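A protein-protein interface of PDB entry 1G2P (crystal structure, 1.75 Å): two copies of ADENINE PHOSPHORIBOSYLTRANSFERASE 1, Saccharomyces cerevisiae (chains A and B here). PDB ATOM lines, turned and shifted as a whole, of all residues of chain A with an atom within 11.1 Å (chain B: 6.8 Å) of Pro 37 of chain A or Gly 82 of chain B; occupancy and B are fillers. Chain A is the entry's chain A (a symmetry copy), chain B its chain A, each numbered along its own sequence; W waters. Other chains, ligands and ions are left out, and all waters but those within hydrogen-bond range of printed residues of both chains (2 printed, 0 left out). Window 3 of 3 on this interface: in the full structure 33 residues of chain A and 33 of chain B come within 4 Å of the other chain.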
ATOM      1  N   TYR A   6      31.653  27.754  -4.205  1.00  0.00           N
ATOM      2  CA  TYR A   6      30.843  26.601  -3.842  1.00  0.00           C
ATOM      3  C   TYR A   6      29.966  26.981  -2.660  1.00  0.00           C
ATOM      4  O   TYR A   6      28.776  26.672  -2.625  1.00  0.00           O
ATOM      5  CB  TYR A   6      31.729  25.411  -3.464  1.00  0.00           C
ATOM      6  CG  TYR A   6      32.350  24.694  -4.643  1.00  0.00           C
ATOM      7  CD1 TYR A   6      33.190  23.596  -4.444  1.00  0.00           C
ATOM      8  CD2 TYR A   6      32.110  25.116  -5.955  1.00  0.00           C
ATOM      9  CE1 TYR A   6      33.778  22.935  -5.522  1.00  0.00           C
ATOM     10  CE2 TYR A   6      32.690  24.463  -7.038  1.00  0.00           C
ATOM     11  CZ  TYR A   6      33.526  23.373  -6.814  1.00  0.00           C
ATOM     12  OH  TYR A   6      34.115  22.725  -7.880  1.00  0.00           O
ATOM     13  N   GLU A   9      26.709  28.651  -3.669  1.00  0.00           N
ATOM     14  CA  GLU A   9      25.724  27.746  -4.243  1.00  0.00           C
ATOM     15  C   GLU A   9      25.142  26.862  -3.133  1.00  0.00           C
ATOM     16  O   GLU A   9      23.952  26.537  -3.140  1.00  0.00           O
ATOM     17  CB  GLU A   9      26.383  26.906  -5.336  1.00  0.00           C
ATOM     18  CG  GLU A   9      25.428  26.280  -6.326  1.00  0.00           C
ATOM     19  CD  GLU A   9      26.155  25.666  -7.511  1.00  0.00           C
ATOM     20  OE1 GLU A   9      25.486  25.078  -8.387  1.00  0.00           O
ATOM     21  OE2 GLU A   9      27.399  25.771  -7.565  1.00  0.00           O
ATOM     22  N   LEU A  10      25.976  26.497  -2.162  1.00  0.00           N
ATOM     23  CA  LEU A  10      25.513  25.676  -1.045  1.00  0.00           C
ATOM     24  C   LEU A  10      24.571  26.482  -0.148  1.00  0.00           C
ATOM     25  O   LEU A  10      23.557  25.970   0.322  1.00  0.00           O
ATOM     26  CB  LEU A  10      26.714  25.160  -0.236  1.00  0.00           C
ATOM     27  CG  LEU A  10      27.618  24.202  -1.024  1.00  0.00           C
ATOM     28  CD1 LEU A  10      28.882  23.905  -0.218  1.00  0.00           C
ATOM     29  CD2 LEU A  10      26.863  22.904  -1.336  1.00  0.00           C
ATOM     30  N   ALA A  13      21.051  26.571  -1.429  1.00  0.00           N
ATOM     31  CA  ALA A  13      20.310  25.314  -1.345  1.00  0.00           C
ATOM     32  C   ALA A  13      19.703  25.076   0.030  1.00  0.00           C
ATOM     33  O   ALA A  13      18.839  24.207   0.192  1.00  0.00           O
ATOM     34  CB  ALA A  13      21.225  24.148  -1.723  1.00  0.00           C
ATOM     35  N   PHE A  30      20.195  21.718   5.933  1.00  0.00           N
ATOM     36  CA  PHE A  30      21.106  21.500   4.812  1.00  0.00           C
ATOM     37  C   PHE A  30      20.778  20.238   4.004  1.00  0.00           C
ATOM     38  O   PHE A  30      21.468  19.918   3.036  1.00  0.00           O
ATOM     39  CB  PHE A  30      22.585  21.481   5.292  1.00  0.00           C
ATOM     40  CG  PHE A  30      23.028  20.200   5.993  1.00  0.00           C
ATOM     41  CD1 PHE A  30      24.388  19.892   6.069  1.00  0.00           C
ATOM     42  CD2 PHE A  30      22.116  19.333   6.600  1.00  0.00           C
ATOM     43  CE1 PHE A  30      24.844  18.737   6.740  1.00  0.00           C
ATOM     44  CE2 PHE A  30      22.558  18.175   7.275  1.00  0.00           C
ATOM     45  CZ  PHE A  30      23.922  17.879   7.345  1.00  0.00           C
ATOM     46  N   LEU A  31      19.715  19.527   4.369  1.00  0.00           N
ATOM     47  CA  LEU A  31      19.376  18.307   3.630  1.00  0.00           C
ATOM     48  C   LEU A  31      19.222  18.409   2.105  1.00  0.00           C
ATOM     49  O   LEU A  31      19.536  17.450   1.389  1.00  0.00           O
ATOM     50  CB  LEU A  31      18.135  17.645   4.232  1.00  0.00           C
ATOM     51  CG  LEU A  31      18.361  17.096   5.642  1.00  0.00           C
ATOM     52  CD1 LEU A  31      17.033  16.572   6.192  1.00  0.00           C
ATOM     53  CD2 LEU A  31      19.410  15.977   5.624  1.00  0.00           C
ATOM     54  N   PRO A  32      18.720  19.547   1.577  1.00  0.00           N
ATOM     55  CA  PRO A  32      18.582  19.638   0.114  1.00  0.00           C
ATOM     56  C   PRO A  32      19.914  19.446  -0.604  1.00  0.00           C
ATOM     57  O   PRO A  32      19.964  19.039  -1.770  1.00  0.00           O
ATOM     58  CB  PRO A  32      18.013  21.050  -0.101  1.00  0.00           C
ATOM     59  CG  PRO A  32      17.238  21.287   1.158  1.00  0.00           C
ATOM     60  CD  PRO A  32      18.153  20.737   2.233  1.00  0.00           C
ATOM     61  N   ILE A  33      21.004  19.740   0.094  1.00  0.00           N
ATOM     62  CA  ILE A  33      22.328  19.591  -0.490  1.00  0.00           C
ATOM     63  C   ILE A  33      22.597  18.137  -0.869  1.00  0.00           C
ATOM     64  O   ILE A  33      23.169  17.863  -1.924  1.00  0.00           O
ATOM     65  CB  ILE A  33      23.421  20.083   0.490  1.00  0.00           C
ATOM     66  CG1 ILE A  33      23.394  21.618   0.565  1.00  0.00           C
ATOM     67  CG2 ILE A  33      24.794  19.586   0.049  1.00  0.00           C
ATOM     68  CD1 ILE A  33      24.297  22.186   1.668  1.00  0.00           C
ATOM     69  N   PHE A  34      22.170  17.210  -0.022  1.00  0.00           N
ATOM     70  CA  PHE A  34      22.397  15.792  -0.280  1.00  0.00           C
ATOM     71  C   PHE A  34      21.493  15.204  -1.366  1.00  0.00           C
ATOM     72  O   PHE A  34      21.804  14.164  -1.942  1.00  0.00           O
ATOM     73  CB  PHE A  34      22.247  15.006   1.020  1.00  0.00           C
ATOM     74  CG  PHE A  34      23.183  15.455   2.096  1.00  0.00           C
ATOM     75  CD1 PHE A  34      22.816  16.466   2.982  1.00  0.00           C
ATOM     76  CD2 PHE A  34      24.452  14.910   2.196  1.00  0.00           C
ATOM     77  CE1 PHE A  34      23.705  16.929   3.949  1.00  0.00           C
ATOM     78  CE2 PHE A  34      25.357  15.364   3.162  1.00  0.00           C
ATOM     79  CZ  PHE A  34      24.987  16.375   4.041  1.00  0.00           C
ATOM     80  N   ARG A  35      20.388  15.880  -1.663  1.00  0.00           N
ATOM     81  CA  ARG A  35      19.462  15.404  -2.686  1.00  0.00           C
ATOM     82  C   ARG A  35      20.047  15.562  -4.083  1.00  0.00           C
ATOM     83  O   ARG A  35      19.594  14.923  -5.033  1.00  0.00           O
ATOM     84  CB  ARG A  35      18.157  16.202  -2.626  1.00  0.00           C
ATOM     85  CG  ARG A  35      17.407  16.130  -1.305  1.00  0.00           C
ATOM     86  CD  ARG A  35      16.166  17.035  -1.359  1.00  0.00           C
ATOM     87  NE  ARG A  35      15.561  17.230  -0.043  1.00  0.00           N
ATOM     88  CZ  ARG A  35      14.654  18.165   0.231  1.00  0.00           C
ATOM     89  NH1 ARG A  35      14.244  18.998  -0.723  1.00  0.00           N
ATOM     90  NH2 ARG A  35      14.157  18.271   1.458  1.00  0.00           N
ATOM     91  N   ASN A  36      21.045  16.427  -4.203  1.00  0.00           N
ATOM     92  CA  ASN A  36      21.678  16.724  -5.483  1.00  0.00           C
ATOM     93  C   ASN A  36      23.143  16.309  -5.401  1.00  0.00           C
ATOM     94  O   ASN A  36      23.928  16.945  -4.707  1.00  0.00           O
ATOM     95  CB  ASN A  36      21.563  18.230  -5.733  1.00  0.00           C
ATOM     96  CG  ASN A  36      22.057  18.646  -7.091  1.00  0.00           C
ATOM     97  OD1 ASN A  36      23.172  18.322  -7.495  1.00  0.00           O
ATOM     98  ND2 ASN A  36      21.224  19.398  -7.806  1.00  0.00           N
ATOM     99  N   PRO A  37      23.537  15.254  -6.137  1.00  0.00           N
ATOM    100  CA  PRO A  37      24.930  14.805  -6.081  1.00  0.00           C
ATOM    101  C   PRO A  37      25.964  15.859  -6.456  1.00  0.00           C
ATOM    102  O   PRO A  37      27.093  15.839  -5.958  1.00  0.00           O
ATOM    103  CB  PRO A  37      24.943  13.572  -6.991  1.00  0.00           C
ATOM    104  CG  PRO A  37      23.794  13.834  -7.954  1.00  0.00           C
ATOM    105  CD  PRO A  37      22.739  14.403  -7.040  1.00  0.00           C
ATOM    106  N   GLY A  38      25.584  16.784  -7.327  1.00  0.00           N
ATOM    107  CA  GLY A  38      26.511  17.831  -7.707  1.00  0.00           C
ATOM    108  C   GLY A  38      26.765  18.768  -6.541  1.00  0.00           C
ATOM    109  O   GLY A  38      27.899  19.185  -6.306  1.00  0.00           O
ATOM    110  N   LEU A  39      25.714  19.094  -5.798  1.00  0.00           N
ATOM    111  CA  LEU A  39      25.841  19.973  -4.644  1.00  0.00           C
ATOM    112  C   LEU A  39      26.577  19.254  -3.509  1.00  0.00           C
ATOM    113  O   LEU A  39      27.413  19.844  -2.810  1.00  0.00           O
ATOM    114  CB  LEU A  39      24.462  20.419  -4.162  1.00  0.00           C
ATOM    115  CG  LEU A  39      23.716  21.457  -5.011  1.00  0.00           C
ATOM    116  CD1 LEU A  39      22.346  21.702  -4.390  1.00  0.00           C
ATOM    117  CD2 LEU A  39      24.519  22.782  -5.084  1.00  0.00           C
ATOM    118  N   PHE A  40      26.268  17.971  -3.345  1.00  0.00           N
ATOM    119  CA  PHE A  40      26.898  17.157  -2.302  1.00  0.00           C
ATOM    120  C   PHE A  40      28.400  17.087  -2.569  1.00  0.00           C
ATOM    121  O   PHE A  40      29.213  17.283  -1.666  1.00  0.00           O
ATOM    122  CB  PHE A  40      26.262  15.754  -2.308  1.00  0.00           C
ATOM    123  CG  PHE A  40      26.703  14.847  -1.164  1.00  0.00           C
ATOM    124  CD1 PHE A  40      26.358  13.499  -1.178  1.00  0.00           C
ATOM    125  CD2 PHE A  40      27.439  15.340  -0.083  1.00  0.00           C
ATOM    126  CE1 PHE A  40      26.744  12.639  -0.125  1.00  0.00           C
ATOM    127  CE2 PHE A  40      27.828  14.498   0.970  1.00  0.00           C
ATOM    128  CZ  PHE A  40      27.475  13.139   0.942  1.00  0.00           C
ATOM    129  N   GLN A  41      28.780  16.820  -3.818  1.00  0.00           N
ATOM    130  CA  GLN A  41      30.190  16.743  -4.145  1.00  0.00           C
ATOM    131  C   GLN A  41      30.880  18.061  -3.835  1.00  0.00           C
ATOM    132  O   GLN A  41      32.029  18.067  -3.393  1.00  0.00           O
ATOM    133  CB  GLN A  41      30.392  16.409  -5.626  1.00  0.00           C
ATOM    134  CG  GLN A  41      31.848  16.123  -5.998  1.00  0.00           C
ATOM    135  CD  GLN A  41      32.404  14.915  -5.266  1.00  0.00           C
ATOM    136  OE1 GLN A  41      33.307  15.034  -4.419  1.00  0.00           O
ATOM    137  NE2 GLN A  41      31.864  13.753  -5.567  1.00  0.00           N
ATOM    138  N   LYS A  42      30.195  19.180  -4.087  1.00  0.00           N
ATOM    139  CA  LYS A  42      30.789  20.487  -3.824  1.00  0.00           C
ATOM    140  C   LYS A  42      31.025  20.710  -2.341  1.00  0.00           C
ATOM    141  O   LYS A  42      32.035  21.308  -1.942  1.00  0.00           O
ATOM    142  CB  LYS A  42      29.916  21.610  -4.418  1.00  0.00           C
ATOM    143  CG  LYS A  42      30.091  21.715  -5.925  1.00  0.00           C
ATOM    144  CD  LYS A  42      29.108  22.661  -6.589  1.00  0.00           C
ATOM    145  CE  LYS A  42      29.308  22.603  -8.115  1.00  0.00           C
ATOM    146  NZ  LYS A  42      28.245  23.329  -8.864  1.00  0.00           N
ATOM    147  N   LEU A  43      30.103  20.225  -1.521  1.00  0.00           N
ATOM    148  CA  LEU A  43      30.243  20.346  -0.077  1.00  0.00           C
ATOM    149  C   LEU A  43      31.500  19.589   0.360  1.00  0.00           C
ATOM    150  O   LEU A  43      32.311  20.099   1.134  1.00  0.00           O
ATOM    151  CB  LEU A  43      29.024  19.748   0.629  1.00  0.00           C
ATOM    152  CG  LEU A  43      29.079  19.759   2.161  1.00  0.00           C
ATOM    153  CD1 LEU A  43      28.431  21.030   2.677  1.00  0.00           C
ATOM    154  CD2 LEU A  43      28.343  18.544   2.726  1.00  0.00           C
ATOM    155  N   ILE A  44      31.644  18.358  -0.121  1.00  0.00           N
ATOM    156  CA  ILE A  44      32.807  17.534   0.211  1.00  0.00           C
ATOM    157  C   ILE A  44      34.099  18.188  -0.313  1.00  0.00           C
ATOM    158  O   ILE A  44      35.113  18.251   0.382  1.00  0.00           O
ATOM    159  CB  ILE A  44      32.666  16.117  -0.401  1.00  0.00           C
ATOM    160  CG1 ILE A  44      31.429  15.417   0.192  1.00  0.00           C
ATOM    161  CG2 ILE A  44      33.957  15.319  -0.205  1.00  0.00           C
ATOM    162  CD1 ILE A  44      31.453  15.217   1.713  1.00  0.00           C
ATOM    163  N   ASP A  45      34.060  18.675  -1.546  1.00  0.00           N
ATOM    164  CA  ASP A  45      35.235  19.306  -2.122  1.00  0.00           C
ATOM    165  C   ASP A  45      35.655  20.538  -1.314  1.00  0.00           C
ATOM    166  O   ASP A  45      36.847  20.790  -1.124  1.00  0.00           O
ATOM    167  CB  ASP A  45      34.964  19.734  -3.567  1.00  0.00           C
ATOM    168  CG  ASP A  45      34.873  18.563  -4.541  1.00  0.00           C
ATOM    169  OD1 ASP A  45      35.153  17.406  -4.171  1.00  0.00           O
ATOM    170  OD2 ASP A  45      34.512  18.815  -5.707  1.00  0.00           O
ATOM    171  N   ALA A  46      34.675  21.311  -0.856  1.00  0.00           N
ATOM    172  CA  ALA A  46      34.955  22.522  -0.098  1.00  0.00           C
ATOM    173  C   ALA A  46      35.665  22.183   1.211  1.00  0.00           C
ATOM    174  O   ALA A  46      36.655  22.812   1.565  1.00  0.00           O
ATOM    175  CB  ALA A  46      33.666  23.275   0.170  1.00  0.00           C
ATOM    176  N   LEU A  72      26.017  12.465   8.090  1.00  0.00           N
ATOM    177  CA  LEU A  72      25.596  12.635   6.704  1.00  0.00           C
ATOM    178  C   LEU A  72      26.718  13.014   5.741  1.00  0.00           C
ATOM    179  O   LEU A  72      26.679  12.622   4.572  1.00  0.00           O
ATOM    180  CB  LEU A  72      24.441  13.649   6.627  1.00  0.00           C
ATOM    181  CG  LEU A  72      23.147  13.182   7.316  1.00  0.00           C
ATOM    182  CD1 LEU A  72      22.220  14.376   7.507  1.00  0.00           C
ATOM    183  CD2 LEU A  72      22.465  12.069   6.496  1.00  0.00           C
ATOM    184  N   THR A  76      31.729  10.475   4.227  1.00  0.00           N
ATOM    185  CA  THR A  76      32.074  10.762   2.830  1.00  0.00           C
ATOM    186  C   THR A  76      33.344  11.621   2.731  1.00  0.00           C
ATOM    187  O   THR A  76      34.195  11.417   1.850  1.00  0.00           O
ATOM    188  CB  THR A  76      30.883  11.467   2.103  1.00  0.00           C
ATOM    189  OG1 THR A  76      29.706  10.648   2.234  1.00  0.00           O
ATOM    190  CG2 THR A  76      31.192  11.660   0.599  1.00  0.00           C
ATOM    191  N   LYS B  48      27.525  -0.809  -4.796  1.00  0.00           N
ATOM    192  CA  LYS B  48      27.411  -0.247  -6.136  1.00  0.00           C
ATOM    193  C   LYS B  48      27.386  -1.351  -7.181  1.00  0.00           C
ATOM    194  O   LYS B  48      26.590  -1.319  -8.113  1.00  0.00           O
ATOM    195  CB  LYS B  48      28.572   0.713  -6.401  1.00  0.00           C
ATOM    196  CG  LYS B  48      28.577   1.344  -7.792  1.00  0.00           C
ATOM    197  CD  LYS B  48      29.494   2.573  -7.815  1.00  0.00           C
ATOM    198  CE  LYS B  48      29.609   3.161  -9.219  1.00  0.00           C
ATOM    199  NZ  LYS B  48      30.337   2.230 -10.129  1.00  0.00           N
ATOM    200  N   LYS B  59      17.088   3.341 -13.746  1.00  0.00           N
ATOM    201  CA  LYS B  59      17.762   4.455 -13.099  1.00  0.00           C
ATOM    202  C   LYS B  59      17.308   4.570 -11.652  1.00  0.00           C
ATOM    203  O   LYS B  59      16.115   4.513 -11.367  1.00  0.00           O
ATOM    204  CB  LYS B  59      17.433   5.746 -13.848  1.00  0.00           C
ATOM    205  CG  LYS B  59      18.031   7.027 -13.249  1.00  0.00           C
ATOM    206  CD  LYS B  59      17.788   8.211 -14.184  1.00  0.00           C
ATOM    207  CE  LYS B  59      18.075   9.551 -13.506  1.00  0.00           C
ATOM    208  NZ  LYS B  59      19.457   9.607 -12.958  1.00  0.00           N
ATOM    209  N   ILE B  60      18.266   4.704 -10.740  1.00  0.00           N
ATOM    210  CA  ILE B  60      17.955   4.865  -9.324  1.00  0.00           C
ATOM    211  C   ILE B  60      17.998   6.365  -9.108  1.00  0.00           C
ATOM    212  O   ILE B  60      18.984   7.011  -9.476  1.00  0.00           O
ATOM    213  CB  ILE B  60      19.018   4.178  -8.433  1.00  0.00           C
ATOM    214  CG1 ILE B  60      18.902   2.650  -8.567  1.00  0.00           C
ATOM    215  CG2 ILE B  60      18.841   4.607  -6.976  1.00  0.00           C
ATOM    216  CD1 ILE B  60      20.054   1.906  -7.926  1.00  0.00           C
ATOM    217  N   ASP B  61      16.929   6.922  -8.544  1.00  0.00           N
ATOM    218  CA  ASP B  61      16.861   8.357  -8.298  1.00  0.00           C
ATOM    219  C   ASP B  61      17.403   8.761  -6.942  1.00  0.00           C
ATOM    220  O   ASP B  61      18.046   9.792  -6.830  1.00  0.00           O
ATOM    221  CB  ASP B  61      15.422   8.856  -8.425  1.00  0.00           C
ATOM    222  CG  ASP B  61      14.907   8.753  -9.842  1.00  0.00           C
ATOM    223  OD1 ASP B  61      15.467   9.441 -10.719  1.00  0.00           O
ATOM    224  OD2 ASP B  61      13.961   7.981 -10.071  1.00  0.00           O
ATOM    225  N   LEU B  77      27.259   6.094  -0.668  1.00  0.00           N
ATOM    226  CA  LEU B  77      26.842   5.228  -1.767  1.00  0.00           C
ATOM    227  C   LEU B  77      26.084   6.045  -2.821  1.00  0.00           C
ATOM    228  O   LEU B  77      26.278   5.866  -4.031  1.00  0.00           O
ATOM    229  CB  LEU B  77      25.943   4.108  -1.232  1.00  0.00           C
ATOM    230  CG  LEU B  77      25.265   3.190  -2.261  1.00  0.00           C
ATOM    231  CD1 LEU B  77      26.326   2.468  -3.100  1.00  0.00           C
ATOM    232  CD2 LEU B  77      24.394   2.170  -1.518  1.00  0.00           C
ATOM    233  N   ALA B  78      25.233   6.953  -2.354  1.00  0.00           N
ATOM    234  CA  ALA B  78      24.458   7.806  -3.255  1.00  0.00           C
ATOM    235  C   ALA B  78      25.434   8.582  -4.143  1.00  0.00           C
ATOM    236  O   ALA B  78      25.291   8.629  -5.359  1.00  0.00           O
ATOM    237  CB  ALA B  78      23.598   8.782  -2.431  1.00  0.00           C
ATOM    238  N   LEU B  79      26.457   9.169  -3.530  1.00  0.00           N
ATOM    239  CA  LEU B  79      27.417   9.947  -4.290  1.00  0.00           C
ATOM    240  C   LEU B  79      28.175   9.060  -5.270  1.00  0.00           C
ATOM    241  O   LEU B  79      28.413   9.462  -6.410  1.00  0.00           O
ATOM    242  CB  LEU B  79      28.368  10.684  -3.331  1.00  0.00           C
ATOM    243  CG  LEU B  79      29.196  11.814  -3.941  1.00  0.00           C
ATOM    244  CD1 LEU B  79      28.276  12.855  -4.598  1.00  0.00           C
ATOM    245  CD2 LEU B  79      30.035  12.465  -2.836  1.00  0.00           C
ATOM    246  N   ALA B  80      28.538   7.852  -4.846  1.00  0.00           N
ATOM    247  CA  ALA B  80      29.245   6.918  -5.717  1.00  0.00           C
ATOM    248  C   ALA B  80      28.388   6.569  -6.930  1.00  0.00           C
ATOM    249  O   ALA B  80      28.906   6.356  -8.018  1.00  0.00           O
ATOM    250  CB  ALA B  80      29.606   5.632  -4.954  1.00  0.00           C
ATOM    251  N   LEU B  81      27.075   6.508  -6.737  1.00  0.00           N
ATOM    252  CA  LEU B  81      26.149   6.186  -7.814  1.00  0.00           C
ATOM    253  C   LEU B  81      25.739   7.393  -8.635  1.00  0.00           C
ATOM    254  O   LEU B  81      25.146   7.237  -9.711  1.00  0.00           O
ATOM    255  CB  LEU B  81      24.886   5.544  -7.246  1.00  0.00           C
ATOM    256  CG  LEU B  81      25.029   4.172  -6.583  1.00  0.00           C
ATOM    257  CD1 LEU B  81      23.772   3.872  -5.762  1.00  0.00           C
ATOM    258  CD2 LEU B  81      25.245   3.097  -7.639  1.00  0.00           C
ATOM    259  N   GLY B  82      26.034   8.589  -8.131  1.00  0.00           N
ATOM    260  CA  GLY B  82      25.663   9.802  -8.841  1.00  0.00           C
ATOM    261  C   GLY B  82      24.182  10.066  -8.667  1.00  0.00           C
ATOM    262  O   GLY B  82      23.510  10.586  -9.558  1.00  0.00           O
ATOM    263  N   VAL B  83      23.658   9.714  -7.502  1.00  0.00           N
ATOM    264  CA  VAL B  83      22.241   9.918  -7.250  1.00  0.00           C
ATOM    265  C   VAL B  83      22.061  10.685  -5.952  1.00  0.00           C
ATOM    266  O   VAL B  83      23.020  10.953  -5.231  1.00  0.00           O
ATOM    267  CB  VAL B  83      21.473   8.568  -7.184  1.00  0.00           C
ATOM    268  CG1 VAL B  83      21.760   7.740  -8.453  1.00  0.00           C
ATOM    269  CG2 VAL B  83      21.866   7.776  -5.913  1.00  0.00           C
ATOM    270  N   GLY B  84      20.824  11.057  -5.664  1.00  0.00           N
ATOM    271  CA  GLY B  84      20.568  11.793  -4.446  1.00  0.00           C
ATOM    272  C   GLY B  84      20.380  10.919  -3.222  1.00  0.00           C
ATOM    273  O   GLY B  84      20.153   9.713  -3.311  1.00  0.00           O
ATOM    274  N   PHE B  85      20.493  11.552  -2.060  1.00  0.00           N
ATOM    275  CA  PHE B  85      20.301  10.886  -0.784  1.00  0.00           C
ATOM    276  C   PHE B  85      19.255  11.656   0.011  1.00  0.00           C
ATOM    277  O   PHE B  85      19.283  12.891   0.050  1.00  0.00           O
ATOM    278  CB  PHE B  85      21.596  10.863   0.035  1.00  0.00           C
ATOM    279  CG  PHE B  85      21.410  10.261   1.399  1.00  0.00           C
ATOM    280  CD1 PHE B  85      21.473   8.883   1.575  1.00  0.00           C
ATOM    281  CD2 PHE B  85      21.063  11.066   2.482  1.00  0.00           C
ATOM    282  CE1 PHE B  85      21.187   8.308   2.807  1.00  0.00           C
ATOM    283  CE2 PHE B  85      20.770  10.505   3.737  1.00  0.00           C
ATOM    284  CZ  PHE B  85      20.831   9.124   3.900  1.00  0.00           C
HETATM  285  O   HOH W   1      23.892  12.943  -3.401  1.00  0.00           O
HETATM  286  O   HOH W   2      18.457  14.925   1.833  1.00  0.00           O
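Gly 84 of chain B touches Phe 34 of chain A (CA to O, 3.7 Å).
Arg 35 of chain A touches Gly 84 of chain B (O to CA, 3.3 Å).
Phe 85 of chain B touches Arg 35 of chain A.
O of Pro 37 of chain A touches CD1 of Leu 79 of chain B, 3.5 Å away.
Pro 37 of chain A touches Gly 82 of chain B.
Val 83 of chain B touches Pro 37 of chain A.
Phe 40 of chain A touches Leu 79 of chain B.
CD2 of Leu 79 of chain B touches NE2 of Gln 41 of chain A (3.5 Å).
Phe 85 of chain B touches Leu 72 of chain A.
Leu 79 of chain B touches Thr 76 of chain A.
Pro 37 of chain A touches three residues of chain B.
Gly 82 of chain B touches just one residue of chain A: Pro 37 (3.6 Å).
No residue of chain A comes within 4 Å of Ala 78 of chain B.
No residue of chain A comes within 4 Å of Ala 80 of chain B.
No residue of chain A comes within 4 Å of Leu 81 of chain B.
Gly 84 of chain B touches two residues of chain A.
Of the printed residues of chain B, Arg 35 of chain A touches Gly 84 and Phe 85.
Of the printed residues of chain B, Thr 76 of chain A touches Leu 79.
Lys 48 of chain B touches none of the printed residues of chain A.
Ile 33 of chain A touches none of the printed residues of chain B.
The nearest residue of chain B that does not touch Pro 37 of chain A is Gly 84 of chain B (4.1 Å).
The nearest printed residue of chain B that does not touch Thr 76 of chain A is Leu 77 of chain B (5.9 Å).
Of the 13 printed residues of chain B, 5 touch a printed residue of chain A.
Printed residues of chain A that touch a printed residue of chain B: Phe 34, Arg 35, Pro 37, Phe 40, Gln 41, Leu 72 and Thr 76.
Among the printed residues, 11 pairs touch across the chains.
Among the printed residues, no Asp or Glu carboxylate lies within 4 Å of a Lys or Arg side-chain nitrogen of the other chain.
No position is printed for both chains.
Of the 11 pairs that touch across the chains among the printed residues, none has its exchanged pair printed and touching as well.
The backbone NH (N) of Phe 85 of chain B is in hydrogen-bond range of the backbone carbonyl oxygen (O) of Phe 34 of chain A (2.9 Å).
Water W2 lies within hydrogen-bond range of the backbone carbonyl oxygen (O) of Leu 31 of chain A and the backbone carbonyl oxygen (O) of Phe 85 of chain B.
Water W1 bridges the backbone carbonyl oxygen of Phe 34 of chain A (2.8 Å) and the backbone carbonyl oxygen of Val 83 of chain B (2.8 Å).
The backbone carbonyl oxygen (O) of Asp 61 of chain B sits at hydrogen-bond distance from the backbone NH (N) of Gly 84 of chain B (3.3 Å).
The side-chain carboxylate (OD1) of Asp 45 of chain A sits close to the side-chain amide oxygen (OE1) of Gln 41 of chain A, 3.0 Å away.
O of Ala 78 of chain B sits at hydrogen-bond distance from N of Val 83 of chain B.
The backbone carbonyl oxygen (O) of Ile 33 of chain A lies within hydrogen-bond range of the backbone NH (N) of Phe 40 of chain A, 3.4 Å away.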
